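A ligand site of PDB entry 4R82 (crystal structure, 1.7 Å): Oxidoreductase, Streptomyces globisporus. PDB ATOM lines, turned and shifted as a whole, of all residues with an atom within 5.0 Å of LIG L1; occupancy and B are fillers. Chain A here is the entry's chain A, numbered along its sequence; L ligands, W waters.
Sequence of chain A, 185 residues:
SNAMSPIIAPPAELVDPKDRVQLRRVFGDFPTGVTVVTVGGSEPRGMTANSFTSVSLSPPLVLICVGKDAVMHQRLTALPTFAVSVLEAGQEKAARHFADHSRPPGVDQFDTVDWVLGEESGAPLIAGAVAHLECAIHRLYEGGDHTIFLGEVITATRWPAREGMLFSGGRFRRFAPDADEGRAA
The backbone NH of Ser 51 lies within hydrogen-bond range of an oxygen (O2) of LIG L1, 3.0 Å away.
OG of Ser 51 sits at hydrogen-bond distance from O2 of LIG L1 (2.8 Å).
A nitrogen (N3) of LIG L1 sits at hydrogen-bond distance from the backbone NH of Asn 50 (3.0 Å).
O3 of LIG L1 lies within hydrogen-bond range of O of Thr 48 (2.8 Å).
A ring nitrogen (NE2) of His 146 is in hydrogen-bond range of a nitrogen (N4) of LG2 L2, 2.8 Å away.
The side-chain amide oxygen of Asn 50 sits close to a nitrogen (N3) of LIG L1, 3.2 Å away.
N of Gly 67 sits at hydrogen-bond distance from O1 of LIG L1 (2.8 Å).
A ring nitrogen (ND1) of His 101 lies within hydrogen-bond range of an oxygen (O6) of LIG L1.
A nitrogen (N2) of LIG L1 is in hydrogen-bond range of the backbone carbonyl oxygen (O) of Cys 65 (2.9 Å).
An oxygen (O4) of LIG L1 sits at hydrogen-bond distance from the backbone carbonyl oxygen of Ala 99, 2.6 Å away.
A nitrogen (N2) of LIG L1 sits close to a nitrogen (N4) of LG2 L2, 3.4 Å away.
The side-chain hydroxyl of Ser 51 lies within hydrogen-bond range of the backbone NH of Cys 65 (2.8 Å).
The backbone carbonyl oxygen (O) of Ala 95 is in hydrogen-bond range of the side-chain hydroxyl (OG1) of Thr 48, at 2.7 Å.
The backbone NH (N) of Thr 48 sits at hydrogen-bond distance from the backbone carbonyl oxygen (O) of Phe 98 (2.9 Å).
N of Ala 99 is in hydrogen-bond range of OG1 of Thr 48, at 3.2 Å.
Merely in contact with LIG L1: Met 47 (3.4 Å), Ala 49 (3.2 Å), Val 66 (3.4 Å), Ala 70 (3.4 Å), Phe 98 (3.8 Å), His 146 (3.9 Å), Phe 167 (3.7 Å) and Phe 172 (3.8 Å).
Hydrophobic or aromatic side chains within 4 Å of LIG L1: Met 47, Ala 49, Ala 70, Ala 99, His 101, Phe 167 and Phe 172.
15 residues have an atom within 4 Å of LIG L1: Met 47, Thr 48, Ala 49, Asn 50, Ser 51, Cys 65, Val 66, Gly 67, Ala 70, Phe 98, Ala 99, His 101, His 146, Phe 167 and Phe 172.
The nearest printed residue that does not touch LIG L1 is Val 71 (4.1 Å).
Water W2 lies within hydrogen-bond range of O9 of LIG L1 (2.7 Å) and N of Val 71 (3.5 Å).
Water W3 lies within hydrogen-bond range of the backbone carbonyl oxygen (O) of Phe 98 (3.0 Å), the backbone carbonyl oxygen (O) of Asp 100 (3.1 Å) and an oxygen (O9) of LIG L1 (3.2 Å).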
ATOM      1  N   VAL A  34      -1.194 -14.955 -14.778  1.00  0.00           N
ATOM      2  CA  VAL A  34      -2.581 -15.357 -14.964  1.00  0.00           C
ATOM      3  C   VAL A  34      -2.678 -16.818 -14.561  1.00  0.00           C
ATOM      4  O   VAL A  34      -1.836 -17.612 -14.956  1.00  0.00           O
ATOM      5  CB  VAL A  34      -2.994 -15.225 -16.442  1.00  0.00           C
ATOM      6  CG1 VAL A  34      -4.468 -15.563 -16.608  1.00  0.00           C
ATOM      7  CG2 VAL A  34      -2.720 -13.819 -16.961  1.00  0.00           C
ATOM      8  N   MET A  47     -11.961 -21.139 -13.696  1.00  0.00           N
ATOM      9  CA  MET A  47     -12.147 -19.692 -13.837  1.00  0.00           C
ATOM     10  C   MET A  47     -10.797 -19.019 -13.906  1.00  0.00           C
ATOM     11  O   MET A  47      -9.922 -19.282 -13.092  1.00  0.00           O
ATOM     12  CB  MET A  47     -12.934 -19.104 -12.657  1.00  0.00           C
ATOM     13  CG  MET A  47     -13.324 -17.608 -12.859  1.00  0.00           C
ATOM     14  SD  MET A  47     -13.939 -16.724 -11.210  1.00  0.00           S
ATOM     15  CE  MET A  47     -12.189 -16.448 -10.409  1.00  0.00           C
ATOM     16  N   THR A  48     -10.628 -18.150 -14.892  1.00  0.00           N
ATOM     17  CA  THR A  48      -9.373 -17.406 -15.016  1.00  0.00           C
ATOM     18  C   THR A  48      -9.259 -16.405 -13.864  1.00  0.00           C
ATOM     19  O   THR A  48     -10.242 -15.722 -13.513  1.00  0.00           O
ATOM     20  CB  THR A  48      -9.317 -16.702 -16.377  1.00  0.00           C
ATOM     21  OG1 THR A  48      -9.350 -17.689 -17.410  1.00  0.00           O
ATOM     22  CG2 THR A  48      -8.046 -15.879 -16.496  1.00  0.00           C
ATOM     23  N   ALA A  49      -8.092 -16.365 -13.239  1.00  0.00           N
ATOM     24  CA  ALA A  49      -7.889 -15.516 -12.058  1.00  0.00           C
ATOM     25  C   ALA A  49      -6.503 -14.919 -12.002  1.00  0.00           C
ATOM     26  O   ALA A  49      -5.496 -15.649 -12.099  1.00  0.00           O
ATOM     27  CB  ALA A  49      -8.166 -16.297 -10.769  1.00  0.00           C
ATOM     28  N   ASN A  50      -6.423 -13.612 -11.785  1.00  0.00           N
ATOM     29  CA  ASN A  50      -5.121 -12.986 -11.568  1.00  0.00           C
ATOM     30  C   ASN A  50      -4.932 -12.477 -10.134  1.00  0.00           C
ATOM     31  O   ASN A  50      -3.884 -11.937  -9.800  1.00  0.00           O
ATOM     32  CB  ASN A  50      -4.886 -11.872 -12.589  1.00  0.00           C
ATOM     33  CG  ASN A  50      -5.643 -10.621 -12.253  1.00  0.00           C
ATOM     34  OD1 ASN A  50      -6.732 -10.668 -11.683  1.00  0.00           O
ATOM     35  ND2 ASN A  50      -5.053  -9.465 -12.570  1.00  0.00           N
ATOM     36  N   SER A  51      -5.943 -12.669  -9.290  1.00  0.00           N
ATOM     37  CA  SER A  51      -5.885 -12.223  -7.900  1.00  0.00           C
ATOM     38  C   SER A  51      -5.081 -13.195  -7.021  1.00  0.00           C
ATOM     39  O   SER A  51      -4.976 -12.991  -5.815  1.00  0.00           O
ATOM     40  CB  SER A  51      -7.287 -12.049  -7.333  1.00  0.00           C
ATOM     41  OG  SER A  51      -7.958 -13.309  -7.297  1.00  0.00           O
ATOM     42  N   CYS A  65      -9.026 -14.116  -4.876  1.00  0.00           N
ATOM     43  CA  CYS A  65     -10.196 -13.276  -4.640  1.00  0.00           C
ATOM     44  C   CYS A  65     -11.172 -13.575  -5.744  1.00  0.00           C
ATOM     45  O   CYS A  65     -10.805 -13.489  -6.920  1.00  0.00           O
ATOM     46  CB  CYS A  65      -9.816 -11.798  -4.701  1.00  0.00           C
ATOM     47  SG  CYS A  65      -8.539 -11.346  -3.491  1.00  0.00           S
ATOM     48  N   VAL A  66     -12.403 -13.914  -5.377  1.00  0.00           N
ATOM     49  CA  VAL A  66     -13.394 -14.374  -6.353  1.00  0.00           C
ATOM     50  C   VAL A  66     -14.675 -13.573  -6.189  1.00  0.00           C
ATOM     51  O   VAL A  66     -15.219 -13.465  -5.076  1.00  0.00           O
ATOM     52  CB  VAL A  66     -13.689 -15.887  -6.176  1.00  0.00           C
ATOM     53  CG1 VAL A  66     -14.737 -16.350  -7.175  1.00  0.00           C
ATOM     54  CG2 VAL A  66     -12.408 -16.693  -6.370  1.00  0.00           C
ATOM     55  N   GLY A  67     -15.155 -13.007  -7.297  1.00  0.00           N
ATOM     56  CA  GLY A  67     -16.367 -12.220  -7.272  1.00  0.00           C
ATOM     57  C   GLY A  67     -17.557 -12.992  -6.726  1.00  0.00           C
ATOM     58  O   GLY A  67     -17.747 -14.176  -7.046  1.00  0.00           O
ATOM     59  N   ASP A  69     -20.615 -12.957  -7.449  1.00  0.00           N
ATOM     60  CA  ASP A  69     -21.594 -13.411  -8.439  1.00  0.00           C
ATOM     61  C   ASP A  69     -21.055 -14.451  -9.437  1.00  0.00           C
ATOM     62  O   ASP A  69     -21.764 -14.866 -10.343  1.00  0.00           O
ATOM     63  CB  ASP A  69     -22.187 -12.216  -9.179  1.00  0.00           C
ATOM     64  CG  ASP A  69     -23.014 -11.320  -8.271  1.00  0.00           C
ATOM     65  OD1 ASP A  69     -23.659 -11.847  -7.327  1.00  0.00           O
ATOM     66  OD2 ASP A  69     -23.034 -10.091  -8.507  1.00  0.00           O
ATOM     67  N   ALA A  70     -19.808 -14.877  -9.270  1.00  0.00           N
ATOM     68  CA  ALA A  70     -19.275 -15.935 -10.114  1.00  0.00           C
ATOM     69  C   ALA A  70     -19.806 -17.295  -9.662  1.00  0.00           C
ATOM     70  O   ALA A  70     -19.953 -17.532  -8.468  1.00  0.00           O
ATOM     71  CB  ALA A  70     -17.748 -15.928 -10.064  1.00  0.00           C
ATOM     72  N   VAL A  71     -20.077 -18.201 -10.606  1.00  0.00           N
ATOM     73  CA  VAL A  71     -20.420 -19.575 -10.260  1.00  0.00           C
ATOM     74  C   VAL A  71     -19.307 -20.221  -9.450  1.00  0.00           C
ATOM     75  O   VAL A  71     -19.550 -20.991  -8.517  1.00  0.00           O
ATOM     76  CB  VAL A  71     -20.734 -20.426 -11.512  1.00  0.00           C
ATOM     77  CG1 VAL A  71     -20.739 -21.907 -11.178  1.00  0.00           C
ATOM     78  CG2 VAL A  71     -22.069 -20.016 -12.099  1.00  0.00           C
ATOM     79  N   ALA A  95      -6.525 -18.853 -21.174  1.00  0.00           N
ATOM     80  CA  ALA A  95      -6.912 -17.747 -20.307  1.00  0.00           C
ATOM     81  C   ALA A  95      -8.242 -17.154 -20.758  1.00  0.00           C
ATOM     82  O   ALA A  95      -9.130 -16.887 -19.939  1.00  0.00           O
ATOM     83  CB  ALA A  95      -5.837 -16.675 -20.287  1.00  0.00           C
ATOM     84  N   PHE A  98     -11.341 -19.726 -20.080  1.00  0.00           N
ATOM     85  CA  PHE A  98     -11.814 -19.824 -18.710  1.00  0.00           C
ATOM     86  C   PHE A  98     -12.266 -18.501 -18.118  1.00  0.00           C
ATOM     87  O   PHE A  98     -12.674 -18.434 -16.959  1.00  0.00           O
ATOM     88  CB  PHE A  98     -10.762 -20.520 -17.835  1.00  0.00           C
ATOM     89  CG  PHE A  98     -10.678 -22.006 -18.093  1.00  0.00           C
ATOM     90  CD1 PHE A  98     -11.673 -22.860 -17.633  1.00  0.00           C
ATOM     91  CD2 PHE A  98      -9.609 -22.529 -18.818  1.00  0.00           C
ATOM     92  CE1 PHE A  98     -11.601 -24.223 -17.878  1.00  0.00           C
ATOM     93  CE2 PHE A  98      -9.540 -23.900 -19.069  1.00  0.00           C
ATOM     94  CZ  PHE A  98     -10.532 -24.746 -18.603  1.00  0.00           C
ATOM     95  N   ALA A  99     -12.207 -17.440 -18.926  1.00  0.00           N
ATOM     96  CA  ALA A  99     -12.786 -16.154 -18.544  1.00  0.00           C
ATOM     97  C   ALA A  99     -14.146 -15.935 -19.190  1.00  0.00           C
ATOM     98  O   ALA A  99     -14.841 -14.944 -18.892  1.00  0.00           O
ATOM     99  CB  ALA A  99     -11.843 -15.020 -18.908  1.00  0.00           C
ATOM    100  N   ASP A 100     -14.518 -16.826 -20.105  1.00  0.00           N
ATOM    101  CA  ASP A 100     -15.789 -16.711 -20.826  1.00  0.00           C
ATOM    102  C   ASP A 100     -16.926 -17.004 -19.870  1.00  0.00           C
ATOM    103  O   ASP A 100     -16.917 -18.015 -19.163  1.00  0.00           O
ATOM    104  CB  ASP A 100     -15.822 -17.682 -22.007  1.00  0.00           C
ATOM    105  CG  ASP A 100     -17.019 -17.461 -22.912  1.00  0.00           C
ATOM    106  OD1 ASP A 100     -17.921 -16.677 -22.546  1.00  0.00           O
ATOM    107  OD2 ASP A 100     -17.065 -18.085 -24.002  1.00  0.00           O
ATOM    108  N   HIS A 101     -17.929 -16.121 -19.845  1.00  0.00           N
ATOM    109  CA  HIS A 101     -19.069 -16.319 -18.950  1.00  0.00           C
ATOM    110  C   HIS A 101     -19.966 -17.468 -19.429  1.00  0.00           C
ATOM    111  O   HIS A 101     -20.610 -18.125 -18.607  1.00  0.00           O
ATOM    112  CB  HIS A 101     -19.886 -15.029 -18.818  1.00  0.00           C
ATOM    113  CG  HIS A 101     -20.963 -15.100 -17.772  1.00  0.00           C
ATOM    114  ND1 HIS A 101     -20.770 -14.680 -16.484  1.00  0.00           N
ATOM    115  CD2 HIS A 101     -22.231 -15.565 -17.838  1.00  0.00           C
ATOM    116  CE1 HIS A 101     -21.887 -14.870 -15.788  1.00  0.00           C
ATOM    117  NE2 HIS A 101     -22.785 -15.400 -16.585  1.00  0.00           N
ATOM    118  N   HIS A 146     -15.932  -9.166  -3.463  1.00  0.00           N
ATOM    119  CA  HIS A 146     -15.276 -10.460  -3.655  1.00  0.00           C
ATOM    120  C   HIS A 146     -15.207 -11.141  -2.314  1.00  0.00           C
ATOM    121  O   HIS A 146     -15.361 -10.507  -1.269  1.00  0.00           O
ATOM    122  CB  HIS A 146     -13.847 -10.291  -4.183  1.00  0.00           C
ATOM    123  CG  HIS A 146     -13.754  -9.955  -5.634  1.00  0.00           C
ATOM    124  ND1 HIS A 146     -14.465  -8.923  -6.212  1.00  0.00           N
ATOM    125  CD2 HIS A 146     -12.996 -10.490  -6.623  1.00  0.00           C
ATOM    126  CE1 HIS A 146     -14.163  -8.848  -7.504  1.00  0.00           C
ATOM    127  NE2 HIS A 146     -13.271  -9.795  -7.778  1.00  0.00           N
ATOM    128  N   PHE A 167      -0.298 -10.270 -17.512  1.00  0.00           N
ATOM    129  CA  PHE A 167      -1.513  -9.476 -17.711  1.00  0.00           C
ATOM    130  C   PHE A 167      -1.215  -8.114 -17.084  1.00  0.00           C
ATOM    131  O   PHE A 167      -0.916  -8.008 -15.887  1.00  0.00           O
ATOM    132  CB  PHE A 167      -2.674 -10.168 -16.968  1.00  0.00           C
ATOM    133  CG  PHE A 167      -4.006  -9.481 -17.103  1.00  0.00           C
ATOM    134  CD1 PHE A 167      -4.529  -9.149 -18.345  1.00  0.00           C
ATOM    135  CD2 PHE A 167      -4.774  -9.229 -15.961  1.00  0.00           C
ATOM    136  CE1 PHE A 167      -5.772  -8.540 -18.449  1.00  0.00           C
ATOM    137  CE2 PHE A 167      -6.019  -8.612 -16.076  1.00  0.00           C
ATOM    138  CZ  PHE A 167      -6.502  -8.274 -17.309  1.00  0.00           C
ATOM    139  N   PHE A 172      -2.832  -8.922 -22.403  1.00  0.00           N
ATOM    140  CA  PHE A 172      -1.869 -10.002 -22.182  1.00  0.00           C
ATOM    141  C   PHE A 172      -0.522  -9.549 -22.748  1.00  0.00           C
ATOM    142  O   PHE A 172      -0.456  -8.898 -23.788  1.00  0.00           O
ATOM    143  CB  PHE A 172      -2.346 -11.295 -22.839  1.00  0.00           C
ATOM    144  CG  PHE A 172      -3.582 -11.884 -22.189  1.00  0.00           C
ATOM    145  CD1 PHE A 172      -3.676 -11.979 -20.806  1.00  0.00           C
ATOM    146  CD2 PHE A 172      -4.647 -12.308 -22.965  1.00  0.00           C
ATOM    147  CE1 PHE A 172      -4.807 -12.525 -20.213  1.00  0.00           C
ATOM    148  CE2 PHE A 172      -5.777 -12.854 -22.371  1.00  0.00           C
ATOM    149  CZ  PHE A 172      -5.852 -12.949 -20.999  1.00  0.00           C
HETATM  150  N1  LIG L   1     -12.570 -13.034 -11.654  1.00  0.00           N
HETATM  151  C1  LIG L   1     -12.410 -13.101 -10.344  1.00  0.00           C
HETATM  152  O1  LIG L   1     -13.542 -13.263  -9.537  1.00  0.00           O
HETATM  153  N2  LIG L   1     -11.235 -13.042  -9.732  1.00  0.00           N
HETATM  154  C2  LIG L   1     -10.119 -12.885 -10.470  1.00  0.00           C
HETATM  155  O2  LIG L   1      -8.883 -12.828  -9.849  1.00  0.00           O
HETATM  156  C3  LIG L   1     -10.220 -12.779 -11.881  1.00  0.00           C
HETATM  157  N3  LIG L   1      -9.087 -12.592 -12.634  1.00  0.00           N
HETATM  158  C4  LIG L   1      -9.204 -12.520 -13.989  1.00  0.00           C
HETATM  159  C5  LIG L   1      -8.036 -12.356 -14.762  1.00  0.00           C
HETATM  160  C6  LIG L   1      -8.147 -12.248 -16.152  1.00  0.00           C
HETATM  161  C7  LIG L   1      -6.881 -12.070 -17.028  1.00  0.00           C
HETATM  162  C8  LIG L   1      -9.410 -12.337 -16.769  1.00  0.00           C
HETATM  163  C9  LIG L   1      -9.499 -12.239 -18.283  1.00  0.00           C
HETATM  164  C10 LIG L   1     -10.568 -12.512 -16.005  1.00  0.00           C
HETATM  165  C11 LIG L   1     -10.471 -12.604 -14.593  1.00  0.00           C
HETATM  166  N4  LIG L   1     -11.615 -12.781 -13.832  1.00  0.00           N
HETATM  167  C12 LIG L   1     -11.477 -12.861 -12.475  1.00  0.00           C
HETATM  168  C13 LIG L   1     -12.953 -12.860 -14.426  1.00  0.00           C
HETATM  169  C14 LIG L   1     -13.447 -14.275 -14.634  1.00  0.00           C
HETATM  170  O3  LIG L   1     -12.398 -15.029 -15.220  1.00  0.00           O
HETATM  171  C15 LIG L   1     -14.603 -14.249 -15.625  1.00  0.00           C
HETATM  172  O4  LIG L   1     -14.206 -13.509 -16.770  1.00  0.00           O
HETATM  173  C16 LIG L   1     -15.789 -13.541 -15.053  1.00  0.00           C
HETATM  174  O5  LIG L   1     -15.942 -13.937 -13.720  1.00  0.00           O
HETATM  175  C17 LIG L   1     -17.071 -13.786 -15.889  1.00  0.00           C
HETATM  176  O6  LIG L   1     -17.619 -15.113 -15.746  1.00  0.00           O
HETATM  177  P1  LIG L   1     -17.848 -15.805 -14.281  1.00  0.00           P
HETATM  178  O7  LIG L   1     -19.042 -16.760 -14.301  1.00  0.00           O
HETATM  179  O8  LIG L   1     -18.101 -14.714 -13.261  1.00  0.00           O
HETATM  180  O9  LIG L   1     -16.608 -16.586 -13.916  1.00  0.00           O
HETATM  181  P1  LG2 L   2     -11.980  -8.581 -20.646  1.00  0.00           P
HETATM  182  O1  LG2 L   2     -11.724  -7.072 -20.762  1.00  0.00           O
HETATM  183  O2  LG2 L   2     -13.228  -8.956 -21.422  1.00  0.00           O
HETATM  184  O3  LG2 L   2     -12.173  -8.993 -19.146  1.00  0.00           O
HETATM  185  C1  LG2 L   2     -13.153  -9.926 -18.886  1.00  0.00           C
HETATM  186  C2  LG2 L   2     -13.811  -9.854 -17.596  1.00  0.00           C
HETATM  187  O4  LG2 L   2     -12.860 -10.158 -16.634  1.00  0.00           O
HETATM  188  C3  LG2 L   2     -14.284  -8.493 -17.299  1.00  0.00           C
HETATM  189  O5  LG2 L   2     -15.665  -8.599 -17.135  1.00  0.00           O
HETATM  190  C4  LG2 L   2     -13.669  -8.120 -16.020  1.00  0.00           C
HETATM  191  O6  LG2 L   2     -14.554  -7.438 -15.194  1.00  0.00           O
HETATM  192  C5  LG2 L   2     -13.299  -9.426 -15.465  1.00  0.00           C
HETATM  193  N1  LG2 L   2     -12.243  -9.421 -14.452  1.00  0.00           N
HETATM  194  C6  LG2 L   2     -10.914  -9.235 -14.615  1.00  0.00           C
HETATM  195  N2  LG2 L   2     -10.296  -9.273 -13.419  1.00  0.00           N
HETATM  196  C7  LG2 L   2     -11.258  -9.511 -12.481  1.00  0.00           C
HETATM  197  C8  LG2 L   2     -11.259  -9.664 -11.097  1.00  0.00           C
HETATM  198  N3  LG2 L   2     -10.075  -9.581 -10.398  1.00  0.00           N
HETATM  199  N4  LG2 L   2     -12.426  -9.896 -10.462  1.00  0.00           N
HETATM  200  C9  LG2 L   2     -13.594  -9.978 -11.117  1.00  0.00           C
HETATM  201  N5  LG2 L   2     -13.618  -9.823 -12.454  1.00  0.00           N
HETATM  202  C10 LG2 L   2     -12.480  -9.611 -13.136  1.00  0.00           C
HETATM  203  O7  LG2 L   2     -10.739  -9.374 -21.233  1.00  0.00           O
HETATM  204  O   HOH W   1     -15.735 -13.115 -11.264  1.00  0.00           O
HETATM  205  O   HOH W   2     -17.057 -18.681 -12.288  1.00  0.00           O
HETATM  206  O   HOH W   3     -15.575 -18.407 -16.362  1.00  0.00           O
